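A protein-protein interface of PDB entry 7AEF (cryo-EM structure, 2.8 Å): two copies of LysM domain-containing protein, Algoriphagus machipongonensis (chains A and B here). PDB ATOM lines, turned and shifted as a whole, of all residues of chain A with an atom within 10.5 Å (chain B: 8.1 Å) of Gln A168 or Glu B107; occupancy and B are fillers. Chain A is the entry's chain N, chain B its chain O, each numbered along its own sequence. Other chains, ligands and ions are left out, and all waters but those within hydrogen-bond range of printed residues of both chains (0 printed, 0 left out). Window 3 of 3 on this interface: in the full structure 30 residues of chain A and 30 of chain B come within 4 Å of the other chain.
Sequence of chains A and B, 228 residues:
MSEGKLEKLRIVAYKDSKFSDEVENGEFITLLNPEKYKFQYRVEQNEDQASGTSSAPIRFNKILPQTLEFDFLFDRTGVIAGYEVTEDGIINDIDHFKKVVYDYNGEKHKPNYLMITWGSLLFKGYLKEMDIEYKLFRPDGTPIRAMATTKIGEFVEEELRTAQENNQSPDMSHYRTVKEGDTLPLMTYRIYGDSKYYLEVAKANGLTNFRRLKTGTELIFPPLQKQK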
ATOM      1  N   THR A 162      -7.089 -27.405   5.475  1.00  0.00           N
ATOM      2  CA  THR A 162      -7.824 -26.977   4.294  1.00  0.00           C
ATOM      3  C   THR A 162      -8.193 -28.133   3.372  1.00  0.00           C
ATOM      4  O   THR A 162      -9.159 -28.013   2.617  1.00  0.00           O
ATOM      5  CB  THR A 162      -7.020 -25.937   3.513  1.00  0.00           C
ATOM      6  OG1 THR A 162      -5.727 -26.461   3.200  1.00  0.00           O
ATOM      7  CG2 THR A 162      -6.856 -24.670   4.323  1.00  0.00           C
ATOM      8  N   ALA A 163      -7.461 -29.246   3.412  1.00  0.00           N
ATOM      9  CA  ALA A 163      -7.845 -30.402   2.614  1.00  0.00           C
ATOM     10  C   ALA A 163      -8.976 -31.188   3.265  1.00  0.00           C
ATOM     11  O   ALA A 163      -9.745 -31.856   2.570  1.00  0.00           O
ATOM     12  CB  ALA A 163      -6.634 -31.300   2.384  1.00  0.00           C
ATOM     13  N   GLN A 164      -9.091 -31.124   4.591  1.00  0.00           N
ATOM     14  CA  GLN A 164     -10.190 -31.787   5.282  1.00  0.00           C
ATOM     15  C   GLN A 164     -11.452 -30.933   5.265  1.00  0.00           C
ATOM     16  O   GLN A 164     -12.562 -31.467   5.195  1.00  0.00           O
ATOM     17  CB  GLN A 164      -9.784 -32.119   6.717  1.00  0.00           C
ATOM     18  CG  GLN A 164      -8.828 -33.284   6.830  1.00  0.00           C
ATOM     19  CD  GLN A 164      -8.196 -33.405   8.201  1.00  0.00           C
ATOM     20  OE1 GLN A 164      -7.802 -32.415   8.808  1.00  0.00           O
ATOM     21  NE2 GLN A 164      -8.096 -34.628   8.695  1.00  0.00           N
ATOM     22  N   GLU A 165     -11.297 -29.614   5.343  1.00  0.00           N
ATOM     23  CA  GLU A 165     -12.388 -28.669   5.115  1.00  0.00           C
ATOM     24  C   GLU A 165     -12.406 -28.335   3.630  1.00  0.00           C
ATOM     25  O   GLU A 165     -11.896 -27.303   3.186  1.00  0.00           O
ATOM     26  CB  GLU A 165     -12.199 -27.405   5.939  1.00  0.00           C
ATOM     27  CG  GLU A 165     -12.177 -27.606   7.423  1.00  0.00           C
ATOM     28  CD  GLU A 165     -11.759 -26.357   8.163  1.00  0.00           C
ATOM     29  OE1 GLU A 165     -11.486 -25.330   7.508  1.00  0.00           O
ATOM     30  OE2 GLU A 165     -11.703 -26.400   9.410  1.00  0.00           O
ATOM     31  N   ASN A 166     -13.001 -29.226   2.843  1.00  0.00           N
ATOM     32  CA  ASN A 166     -13.071 -29.038   1.397  1.00  0.00           C
ATOM     33  C   ASN A 166     -14.120 -27.959   1.122  1.00  0.00           C
ATOM     34  O   ASN A 166     -15.281 -28.226   0.805  1.00  0.00           O
ATOM     35  CB  ASN A 166     -13.379 -30.366   0.712  1.00  0.00           C
ATOM     36  CG  ASN A 166     -13.562 -30.236  -0.777  1.00  0.00           C
ATOM     37  OD1 ASN A 166     -12.867 -29.474  -1.443  1.00  0.00           O
ATOM     38  ND2 ASN A 166     -14.516 -30.978  -1.309  1.00  0.00           N
ATOM     39  N   ASN A 167     -13.695 -26.707   1.273  1.00  0.00           N
ATOM     40  CA  ASN A 167     -14.597 -25.565   1.247  1.00  0.00           C
ATOM     41  C   ASN A 167     -15.002 -25.257  -0.186  1.00  0.00           C
ATOM     42  O   ASN A 167     -14.152 -24.984  -1.037  1.00  0.00           O
ATOM     43  CB  ASN A 167     -13.931 -24.354   1.891  1.00  0.00           C
ATOM     44  CG  ASN A 167     -14.066 -24.352   3.392  1.00  0.00           C
ATOM     45  OD1 ASN A 167     -15.107 -24.706   3.930  1.00  0.00           O
ATOM     46  ND2 ASN A 167     -13.006 -23.971   4.078  1.00  0.00           N
ATOM     47  N   GLN A 168     -16.298 -25.303  -0.458  1.00  0.00           N
ATOM     48  CA  GLN A 168     -16.787 -25.034  -1.799  1.00  0.00           C
ATOM     49  C   GLN A 168     -17.808 -23.904  -1.803  1.00  0.00           C
ATOM     50  O   GLN A 168     -17.449 -22.733  -1.942  1.00  0.00           O
ATOM     51  CB  GLN A 168     -17.390 -26.297  -2.401  1.00  0.00           C
ATOM     52  CG  GLN A 168     -18.806 -26.578  -1.974  1.00  0.00           C
ATOM     53  CD  GLN A 168     -19.145 -28.043  -2.074  1.00  0.00           C
ATOM     54  OE1 GLN A 168     -18.332 -28.902  -1.734  1.00  0.00           O
ATOM     55  NE2 GLN A 168     -20.348 -28.342  -2.543  1.00  0.00           N
ATOM     56  N   PRO A 170     -21.202 -20.876  -5.411  1.00  0.00           N
ATOM     57  CA  PRO A 170     -20.912 -19.486  -5.774  1.00  0.00           C
ATOM     58  C   PRO A 170     -19.422 -19.160  -5.893  1.00  0.00           C
ATOM     59  O   PRO A 170     -19.100 -18.045  -6.279  1.00  0.00           O
ATOM     60  CB  PRO A 170     -21.548 -18.697  -4.628  1.00  0.00           C
ATOM     61  CG  PRO A 170     -22.672 -19.532  -4.193  1.00  0.00           C
ATOM     62  CD  PRO A 170     -22.250 -20.962  -4.379  1.00  0.00           C
ATOM     63  N   ASP A 171     -18.534 -20.100  -5.570  1.00  0.00           N
ATOM     64  CA  ASP A 171     -17.106 -19.904  -5.794  1.00  0.00           C
ATOM     65  C   ASP A 171     -16.493 -20.893  -6.770  1.00  0.00           C
ATOM     66  O   ASP A 171     -15.483 -20.568  -7.400  1.00  0.00           O
ATOM     67  CB  ASP A 171     -16.325 -19.972  -4.477  1.00  0.00           C
ATOM     68  CG  ASP A 171     -16.394 -18.689  -3.688  1.00  0.00           C
ATOM     69  OD1 ASP A 171     -16.491 -17.612  -4.307  1.00  0.00           O
ATOM     70  OD2 ASP A 171     -16.335 -18.748  -2.443  1.00  0.00           O
ATOM     71  N   MET A 172     -17.059 -22.085  -6.918  1.00  0.00           N
ATOM     72  CA  MET A 172     -16.491 -23.110  -7.787  1.00  0.00           C
ATOM     73  C   MET A 172     -17.465 -23.457  -8.902  1.00  0.00           C
ATOM     74  O   MET A 172     -18.574 -22.927  -8.971  1.00  0.00           O
ATOM     75  CB  MET A 172     -16.133 -24.378  -7.003  1.00  0.00           C
ATOM     76  CG  MET A 172     -15.630 -24.152  -5.583  1.00  0.00           C
ATOM     77  SD  MET A 172     -14.081 -23.236  -5.470  1.00  0.00           S
ATOM     78  CE  MET A 172     -13.007 -24.282  -6.429  1.00  0.00           C
ATOM     79  N   SER A 173     -17.039 -24.363  -9.773  1.00  0.00           N
ATOM     80  CA  SER A 173     -17.862 -24.815 -10.886  1.00  0.00           C
ATOM     81  C   SER A 173     -18.569 -26.126 -10.554  1.00  0.00           C
ATOM     82  O   SER A 173     -18.115 -26.911  -9.725  1.00  0.00           O
ATOM     83  CB  SER A 173     -17.009 -24.997 -12.134  1.00  0.00           C
ATOM     84  OG  SER A 173     -16.624 -23.750 -12.663  1.00  0.00           O
ATOM     85  N   HIS A 174     -19.685 -26.362 -11.240  1.00  0.00           N
ATOM     86  CA  HIS A 174     -20.563 -27.482 -10.934  1.00  0.00           C
ATOM     87  C   HIS A 174     -21.199 -27.994 -12.220  1.00  0.00           C
ATOM     88  O   HIS A 174     -21.377 -27.235 -13.170  1.00  0.00           O
ATOM     89  CB  HIS A 174     -21.638 -27.050  -9.930  1.00  0.00           C
ATOM     90  CG  HIS A 174     -22.497 -28.170  -9.440  1.00  0.00           C
ATOM     91  ND1 HIS A 174     -21.983 -29.293  -8.832  1.00  0.00           N
ATOM     92  CD2 HIS A 174     -23.837 -28.339  -9.470  1.00  0.00           C
ATOM     93  CE1 HIS A 174     -22.970 -30.108  -8.510  1.00  0.00           C
ATOM     94  NE2 HIS A 174     -24.105 -29.551  -8.884  1.00  0.00           N
ATOM     95  N   TYR A 175     -21.520 -29.291 -12.256  1.00  0.00           N
ATOM     96  CA  TYR A 175     -22.280 -29.869 -13.358  1.00  0.00           C
ATOM     97  C   TYR A 175     -23.344 -30.821 -12.821  1.00  0.00           C
ATOM     98  O   TYR A 175     -23.147 -31.486 -11.804  1.00  0.00           O
ATOM     99  CB  TYR A 175     -21.362 -30.588 -14.391  1.00  0.00           C
ATOM    100  CG  TYR A 175     -20.517 -31.738 -13.877  1.00  0.00           C
ATOM    101  CD1 TYR A 175     -21.029 -33.030 -13.803  1.00  0.00           C
ATOM    102  CD2 TYR A 175     -19.198 -31.542 -13.505  1.00  0.00           C
ATOM    103  CE1 TYR A 175     -20.268 -34.074 -13.338  1.00  0.00           C
ATOM    104  CE2 TYR A 175     -18.424 -32.588 -13.041  1.00  0.00           C
ATOM    105  CZ  TYR A 175     -18.967 -33.848 -12.958  1.00  0.00           C
ATOM    106  OH  TYR A 175     -18.204 -34.894 -12.502  1.00  0.00           O
ATOM    107  N   ARG A 176     -24.486 -30.864 -13.510  1.00  0.00           N
ATOM    108  CA  ARG A 176     -25.570 -31.793 -13.212  1.00  0.00           C
ATOM    109  C   ARG A 176     -26.110 -32.379 -14.508  1.00  0.00           C
ATOM    110  O   ARG A 176     -25.867 -31.859 -15.596  1.00  0.00           O
ATOM    111  CB  ARG A 176     -26.743 -31.136 -12.469  1.00  0.00           C
ATOM    112  CG  ARG A 176     -26.395 -30.338 -11.246  1.00  0.00           C
ATOM    113  CD  ARG A 176     -27.631 -29.935 -10.503  1.00  0.00           C
ATOM    114  NE  ARG A 176     -28.085 -31.002  -9.628  1.00  0.00           N
ATOM    115  CZ  ARG A 176     -27.715 -31.133  -8.360  1.00  0.00           C
ATOM    116  NH1 ARG A 176     -26.883 -30.260  -7.816  1.00  0.00           N
ATOM    117  NH2 ARG A 176     -28.180 -32.141  -7.637  1.00  0.00           N
ATOM    118  N   MET A 187     -33.579 -25.519  -9.772  1.00  0.00           N
ATOM    119  CA  MET A 187     -32.197 -25.984  -9.671  1.00  0.00           C
ATOM    120  C   MET A 187     -31.242 -24.843  -9.359  1.00  0.00           C
ATOM    121  O   MET A 187     -30.226 -25.047  -8.688  1.00  0.00           O
ATOM    122  CB  MET A 187     -31.774 -26.674 -10.966  1.00  0.00           C
ATOM    123  CG  MET A 187     -32.374 -28.041 -11.180  1.00  0.00           C
ATOM    124  SD  MET A 187     -31.537 -28.966 -12.479  1.00  0.00           S
ATOM    125  CE  MET A 187     -31.903 -27.963 -13.906  1.00  0.00           C
ATOM    126  N   TYR A 189     -31.950 -22.295  -7.486  1.00  0.00           N
ATOM    127  CA  TYR A 189     -32.132 -21.963  -6.079  1.00  0.00           C
ATOM    128  C   TYR A 189     -31.329 -22.893  -5.175  1.00  0.00           C
ATOM    129  O   TYR A 189     -30.819 -22.468  -4.133  1.00  0.00           O
ATOM    130  CB  TYR A 189     -33.614 -22.031  -5.734  1.00  0.00           C
ATOM    131  CG  TYR A 189     -33.917 -21.826  -4.279  1.00  0.00           C
ATOM    132  CD1 TYR A 189     -33.745 -20.585  -3.688  1.00  0.00           C
ATOM    133  CD2 TYR A 189     -34.361 -22.878  -3.491  1.00  0.00           C
ATOM    134  CE1 TYR A 189     -34.018 -20.389  -2.354  1.00  0.00           C
ATOM    135  CE2 TYR A 189     -34.634 -22.695  -2.156  1.00  0.00           C
ATOM    136  CZ  TYR A 189     -34.464 -21.448  -1.597  1.00  0.00           C
ATOM    137  OH  TYR A 189     -34.741 -21.257  -0.265  1.00  0.00           O
ATOM    138  N   ARG A 190     -31.208 -24.162  -5.550  1.00  0.00           N
ATOM    139  CA  ARG A 190     -30.502 -25.112  -4.705  1.00  0.00           C
ATOM    140  C   ARG A 190     -28.993 -25.002  -4.846  1.00  0.00           C
ATOM    141  O   ARG A 190     -28.259 -25.519  -4.000  1.00  0.00           O
ATOM    142  CB  ARG A 190     -30.952 -26.533  -5.029  1.00  0.00           C
ATOM    143  CG  ARG A 190     -32.332 -26.855  -4.528  1.00  0.00           C
ATOM    144  CD  ARG A 190     -32.843 -28.152  -5.105  1.00  0.00           C
ATOM    145  NE  ARG A 190     -34.148 -28.498  -4.555  1.00  0.00           N
ATOM    146  CZ  ARG A 190     -34.860 -29.558  -4.924  1.00  0.00           C
ATOM    147  NH1 ARG A 190     -34.393 -30.384  -5.844  1.00  0.00           N
ATOM    148  NH2 ARG A 190     -36.036 -29.791  -4.366  1.00  0.00           N
ATOM    149  N   ILE A 191     -28.508 -24.349  -5.893  1.00  0.00           N
ATOM    150  CA  ILE A 191     -27.079 -24.244  -6.123  1.00  0.00           C
ATOM    151  C   ILE A 191     -26.545 -22.893  -5.661  1.00  0.00           C
ATOM    152  O   ILE A 191     -25.483 -22.814  -5.041  1.00  0.00           O
ATOM    153  CB  ILE A 191     -26.778 -24.523  -7.613  1.00  0.00           C
ATOM    154  CG1 ILE A 191     -27.019 -26.003  -7.917  1.00  0.00           C
ATOM    155  CG2 ILE A 191     -25.362 -24.154  -7.989  1.00  0.00           C
ATOM    156  CD1 ILE A 191     -27.112 -26.324  -9.371  1.00  0.00           C
ATOM    157  N   TYR A 192     -27.295 -21.823  -5.897  1.00  0.00           N
ATOM    158  CA  TYR A 192     -26.843 -20.482  -5.557  1.00  0.00           C
ATOM    159  C   TYR A 192     -27.515 -19.904  -4.323  1.00  0.00           C
ATOM    160  O   TYR A 192     -26.964 -18.982  -3.718  1.00  0.00           O
ATOM    161  CB  TYR A 192     -27.077 -19.524  -6.731  1.00  0.00           C
ATOM    162  CG  TYR A 192     -26.289 -19.863  -7.968  1.00  0.00           C
ATOM    163  CD1 TYR A 192     -24.940 -19.559  -8.054  1.00  0.00           C
ATOM    164  CD2 TYR A 192     -26.890 -20.487  -9.049  1.00  0.00           C
ATOM    165  CE1 TYR A 192     -24.212 -19.866  -9.175  1.00  0.00           C
ATOM    166  CE2 TYR A 192     -26.169 -20.795 -10.175  1.00  0.00           C
ATOM    167  CZ  TYR A 192     -24.830 -20.484 -10.232  1.00  0.00           C
ATOM    168  OH  TYR A 192     -24.103 -20.787 -11.353  1.00  0.00           O
ATOM    169  N   GLY A 193     -28.681 -20.403  -3.936  1.00  0.00           N
ATOM    170  CA  GLY A 193     -29.448 -19.781  -2.882  1.00  0.00           C
ATOM    171  C   GLY A 193     -30.450 -18.749  -3.346  1.00  0.00           C
ATOM    172  O   GLY A 193     -31.103 -18.128  -2.504  1.00  0.00           O
ATOM    173  N   PRO A 223     -19.351 -20.140 -11.492  1.00  0.00           N
ATOM    174  CA  PRO A 223     -19.376 -19.335 -10.269  1.00  0.00           C
ATOM    175  C   PRO A 223     -19.649 -17.865 -10.558  1.00  0.00           C
ATOM    176  O   PRO A 223     -19.530 -17.387 -11.683  1.00  0.00           O
ATOM    177  CB  PRO A 223     -17.971 -19.528  -9.698  1.00  0.00           C
ATOM    178  CG  PRO A 223     -17.140 -19.783 -10.884  1.00  0.00           C
ATOM    179  CD  PRO A 223     -17.987 -20.592 -11.810  1.00  0.00           C
ATOM    180  N   LEU A 224     -20.015 -17.147  -9.505  1.00  0.00           N
ATOM    181  CA  LEU A 224     -20.243 -15.711  -9.585  1.00  0.00           C
ATOM    182  C   LEU A 224     -18.919 -14.960  -9.593  1.00  0.00           C
ATOM    183  O   LEU A 224     -17.937 -15.390  -8.984  1.00  0.00           O
ATOM    184  CB  LEU A 224     -21.097 -15.248  -8.407  1.00  0.00           C
ATOM    185  CG  LEU A 224     -22.439 -15.963  -8.253  1.00  0.00           C
ATOM    186  CD1 LEU A 224     -23.136 -15.534  -6.989  1.00  0.00           C
ATOM    187  CD2 LEU A 224     -23.312 -15.703  -9.455  1.00  0.00           C
ATOM    188  N   LYS A 226     -16.194 -12.008  -8.732  1.00  0.00           N
ATOM    189  CA  LYS A 226     -15.826 -11.592  -7.383  1.00  0.00           C
ATOM    190  C   LYS A 226     -15.622 -10.091  -7.234  1.00  0.00           C
ATOM    191  O   LYS A 226     -16.024  -9.521  -6.216  1.00  0.00           O
ATOM    192  CB  LYS A 226     -14.562 -12.327  -6.943  1.00  0.00           C
ATOM    193  CG  LYS A 226     -14.813 -13.777  -6.586  1.00  0.00           C
ATOM    194  CD  LYS A 226     -13.639 -14.388  -5.848  1.00  0.00           C
ATOM    195  CE  LYS A 226     -12.436 -14.550  -6.755  1.00  0.00           C
ATOM    196  NZ  LYS A 226     -11.655 -15.764  -6.391  1.00  0.00           N
ATOM    197  N   LYS B  15     -29.505 -29.557   5.884  1.00  0.00           N
ATOM    198  CA  LYS B  15     -28.656 -28.592   5.190  1.00  0.00           C
ATOM    199  C   LYS B  15     -29.115 -27.148   5.313  1.00  0.00           C
ATOM    200  O   LYS B  15     -28.271 -26.248   5.316  1.00  0.00           O
ATOM    201  CB  LYS B  15     -28.558 -28.930   3.703  1.00  0.00           C
ATOM    202  CG  LYS B  15     -27.663 -30.101   3.374  1.00  0.00           C
ATOM    203  CD  LYS B  15     -27.514 -30.257   1.880  1.00  0.00           C
ATOM    204  CE  LYS B  15     -28.781 -30.821   1.276  1.00  0.00           C
ATOM    205  NZ  LYS B  15     -28.640 -31.087  -0.176  1.00  0.00           N
ATOM    206  N   GLU B  22     -32.406 -32.827   3.327  1.00  0.00           N
ATOM    207  CA  GLU B  22     -31.658 -33.751   4.165  1.00  0.00           C
ATOM    208  C   GLU B  22     -30.242 -33.977   3.651  1.00  0.00           C
ATOM    209  O   GLU B  22     -29.998 -34.046   2.446  1.00  0.00           O
ATOM    210  CB  GLU B  22     -32.371 -35.095   4.254  1.00  0.00           C
ATOM    211  CG  GLU B  22     -33.682 -35.052   4.995  1.00  0.00           C
ATOM    212  CD  GLU B  22     -34.304 -36.421   5.135  1.00  0.00           C
ATOM    213  OE1 GLU B  22     -33.553 -37.416   5.172  1.00  0.00           O
ATOM    214  OE2 GLU B  22     -35.547 -36.506   5.200  1.00  0.00           O
ATOM    215  N   VAL B  23     -29.312 -34.099   4.594  1.00  0.00           N
ATOM    216  CA  VAL B  23     -27.964 -34.571   4.306  1.00  0.00           C
ATOM    217  C   VAL B  23     -28.048 -36.046   3.941  1.00  0.00           C
ATOM    218  O   VAL B  23     -28.766 -36.817   4.586  1.00  0.00           O
ATOM    219  CB  VAL B  23     -27.051 -34.329   5.525  1.00  0.00           C
ATOM    220  CG1 VAL B  23     -25.717 -35.061   5.413  1.00  0.00           C
ATOM    221  CG2 VAL B  23     -26.817 -32.852   5.731  1.00  0.00           C
ATOM    222  N   GLU B  24     -27.346 -36.445   2.884  1.00  0.00           N
ATOM    223  CA  GLU B  24     -27.398 -37.829   2.438  1.00  0.00           C
ATOM    224  C   GLU B  24     -26.563 -38.722   3.347  1.00  0.00           C
ATOM    225  O   GLU B  24     -25.411 -38.397   3.657  1.00  0.00           O
ATOM    226  CB  GLU B  24     -26.919 -37.934   0.993  1.00  0.00           C
ATOM    227  CG  GLU B  24     -27.850 -37.258   0.006  1.00  0.00           C
ATOM    228  CD  GLU B  24     -29.199 -37.950  -0.102  1.00  0.00           C
ATOM    229  OE1 GLU B  24     -29.252 -39.189   0.038  1.00  0.00           O
ATOM    230  OE2 GLU B  24     -30.211 -37.250  -0.323  1.00  0.00           O
ATOM    231  N   TYR B 104     -17.465 -31.116  10.521  1.00  0.00           N
ATOM    232  CA  TYR B 104     -17.601 -29.918   9.704  1.00  0.00           C
ATOM    233  C   TYR B 104     -17.978 -30.303   8.274  1.00  0.00           C
ATOM    234  O   TYR B 104     -17.422 -31.242   7.704  1.00  0.00           O
ATOM    235  CB  TYR B 104     -16.275 -29.149   9.759  1.00  0.00           C
ATOM    236  CG  TYR B 104     -16.133 -27.830   9.021  1.00  0.00           C
ATOM    237  CD1 TYR B 104     -16.141 -26.627   9.714  1.00  0.00           C
ATOM    238  CD2 TYR B 104     -15.891 -27.790   7.652  1.00  0.00           C
ATOM    239  CE1 TYR B 104     -15.965 -25.428   9.056  1.00  0.00           C
ATOM    240  CE2 TYR B 104     -15.735 -26.605   6.991  1.00  0.00           C
ATOM    241  CZ  TYR B 104     -15.764 -25.430   7.691  1.00  0.00           C
ATOM    242  OH  TYR B 104     -15.595 -24.253   7.012  1.00  0.00           O
ATOM    243  N   ASN B 105     -18.916 -29.568   7.691  1.00  0.00           N
ATOM    244  CA  ASN B 105     -19.429 -29.834   6.352  1.00  0.00           C
ATOM    245  C   ASN B 105     -18.922 -28.740   5.420  1.00  0.00           C
ATOM    246  O   ASN B 105     -19.231 -27.563   5.615  1.00  0.00           O
ATOM    247  CB  ASN B 105     -20.958 -29.883   6.372  1.00  0.00           C
ATOM    248  CG  ASN B 105     -21.549 -30.594   5.174  1.00  0.00           C
ATOM    249  OD1 ASN B 105     -20.878 -30.818   4.170  1.00  0.00           O
ATOM    250  ND2 ASN B 105     -22.818 -30.951   5.274  1.00  0.00           N
ATOM    251  N   GLY B 106     -18.137 -29.130   4.417  1.00  0.00           N
ATOM    252  CA  GLY B 106     -17.539 -28.172   3.502  1.00  0.00           C
ATOM    253  C   GLY B 106     -18.498 -27.580   2.495  1.00  0.00           C
ATOM    254  O   GLY B 106     -18.159 -26.584   1.852  1.00  0.00           O
ATOM    255  N   GLU B 107     -19.686 -28.161   2.347  1.00  0.00           N
ATOM    256  CA  GLU B 107     -20.690 -27.587   1.462  1.00  0.00           C
ATOM    257  C   GLU B 107     -21.337 -26.350   2.073  1.00  0.00           C
ATOM    258  O   GLU B 107     -21.703 -25.419   1.349  1.00  0.00           O
ATOM    259  CB  GLU B 107     -21.745 -28.637   1.139  1.00  0.00           C
ATOM    260  CG  GLU B 107     -22.557 -28.339  -0.093  1.00  0.00           C
ATOM    261  CD  GLU B 107     -23.792 -29.198  -0.176  1.00  0.00           C
ATOM    262  OE1 GLU B 107     -23.819 -30.254   0.490  1.00  0.00           O
ATOM    263  OE2 GLU B 107     -24.732 -28.825  -0.905  1.00  0.00           O
ATOM    264  N   LYS B 108     -21.493 -26.322   3.396  1.00  0.00           N
ATOM    265  CA  LYS B 108     -22.133 -25.208   4.083  1.00  0.00           C
ATOM    266  C   LYS B 108     -21.198 -24.420   4.983  1.00  0.00           C
ATOM    267  O   LYS B 108     -21.647 -23.439   5.581  1.00  0.00           O
ATOM    268  CB  LYS B 108     -23.314 -25.706   4.920  1.00  0.00           C
ATOM    269  CG  LYS B 108     -24.440 -26.298   4.113  1.00  0.00           C
ATOM    270  CD  LYS B 108     -25.066 -25.271   3.192  1.00  0.00           C
ATOM    271  CE  LYS B 108     -25.922 -25.952   2.143  1.00  0.00           C
ATOM    272  NZ  LYS B 108     -26.483 -24.991   1.162  1.00  0.00           N
ATOM    273  N   HIS B 109     -19.931 -24.840   5.108  1.00  0.00           N
ATOM    274  CA  HIS B 109     -18.887 -24.185   5.908  1.00  0.00           C
ATOM    275  C   HIS B 109     -19.214 -24.164   7.402  1.00  0.00           C
ATOM    276  O   HIS B 109     -18.867 -23.215   8.099  1.00  0.00           O
ATOM    277  CB  HIS B 109     -18.575 -22.763   5.414  1.00  0.00           C
ATOM    278  CG  HIS B 109     -18.428 -22.645   3.930  1.00  0.00           C
ATOM    279  ND1 HIS B 109     -17.207 -22.670   3.302  1.00  0.00           N
ATOM    280  CD2 HIS B 109     -19.350 -22.479   2.953  1.00  0.00           C
ATOM    281  CE1 HIS B 109     -17.382 -22.539   2.000  1.00  0.00           C
ATOM    282  NE2 HIS B 109     -18.674 -22.426   1.763  1.00  0.00           N
ATOM    283  N   LYS B 110     -19.850 -25.230   7.908  1.00  0.00           N
ATOM    284  CA  LYS B 110     -20.302 -25.318   9.297  1.00  0.00           C
ATOM    285  C   LYS B 110     -20.664 -26.760   9.646  1.00  0.00           C
ATOM    286  O   LYS B 110     -20.696 -27.611   8.753  1.00  0.00           O
ATOM    287  CB  LYS B 110     -21.501 -24.390   9.516  1.00  0.00           C
ATOM    288  CG  LYS B 110     -22.579 -24.571   8.488  1.00  0.00           C
ATOM    289  CD  LYS B 110     -23.552 -23.429   8.479  1.00  0.00           C
ATOM    290  CE  LYS B 110     -24.617 -23.643   9.494  1.00  0.00           C
ATOM    291  NZ  LYS B 110     -25.439 -24.830   9.141  1.00  0.00           N
ATOM    292  N   ASN B 112     -23.709 -29.483  11.063  1.00  0.00           N
ATOM    293  CA  ASN B 112     -25.056 -29.715  10.551  1.00  0.00           C
ATOM    294  C   ASN B 112     -26.145 -29.190  11.490  1.00  0.00           C
ATOM    295  O   ASN B 112     -25.955 -29.058  12.699  1.00  0.00           O
ATOM    296  CB  ASN B 112     -25.280 -31.210  10.317  1.00  0.00           C
ATOM    297  CG  ASN B 112     -24.530 -31.743   9.108  1.00  0.00           C
ATOM    298  OD1 ASN B 112     -24.320 -31.033   8.134  1.00  0.00           O
ATOM    299  ND2 ASN B 112     -24.136 -33.003   9.164  1.00  0.00           N
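The side-chain amide oxygen (OD1) of Asn A167 lies within hydrogen-bond range of the side-chain hydroxyl (OH) of Tyr B104 (3.2 Å). The side-chain amide oxygen (OD1) of Asn A167 lies within hydrogen-bond range of a ring nitrogen (ND1) of His B109. The backbone NH (N) of Gln A168 sits at hydrogen-bond distance from the backbone carbonyl oxygen (O) of Gly B106 (3.2 Å). The backbone carbonyl oxygen (O) of Gly B106 lies close to the backbone carbonyl oxygen (O) of Asn A166, 3.5 Å away.
No position is printed for both chains. Of the 8 pairs that touch across the chains among the printed residues, none has its exchanged pair printed and touching as well.
Of the 23 printed residues of chain A, 4 touch a printed residue of chain B. Along chain A the printed residues that touch a printed residue of chain B span positions 165 to 168. Of the 12 printed residues of chain B, 4 touch a printed residue of chain A. Printed residues of chain B that touch a printed residue of chain A: Tyr B104, Gly B106, Glu B107 and His B109. Hydrophobic or aromatic side chains of chain B within 4 Å of the printed part of chain A: Tyr B104 and His B109.
The side-chain amide oxygen (OD1) of Asn B105 sits close to the backbone NH (N) of Glu B107 (3.4 Å).
Of the printed residues of chain B, Asn A166 touches Gly B106. Of the printed residues of chain B, Asn A167 touches Tyr B104 (3.2 Å), Gly B106 (3.8 Å) and His B109 (3.0 Å). Gln A168 touches just these residues of chain B: Gly B106 (3.2 Å), Glu B107 (3.3 Å) and His B109 (3.9 Å). No residue of chain A comes within 4 Å of Asn B105. Gly B106 touches three residues of chain A. Lys B108 touches none of the printed residues of chain A. Printed residues of chain A within 4 Å of His B109: Asn A167 and Gln A168.
Glu A165 touches Tyr B104 (CG to CE2, 3.7 Å). O of Gly B106 touches CA of Asn A167, at 3.8 Å. Gln A168 touches Glu B107 (NE2 to CG, 3.3 Å). Gln A168 touches His B109 (N to CE1, 3.9 Å).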
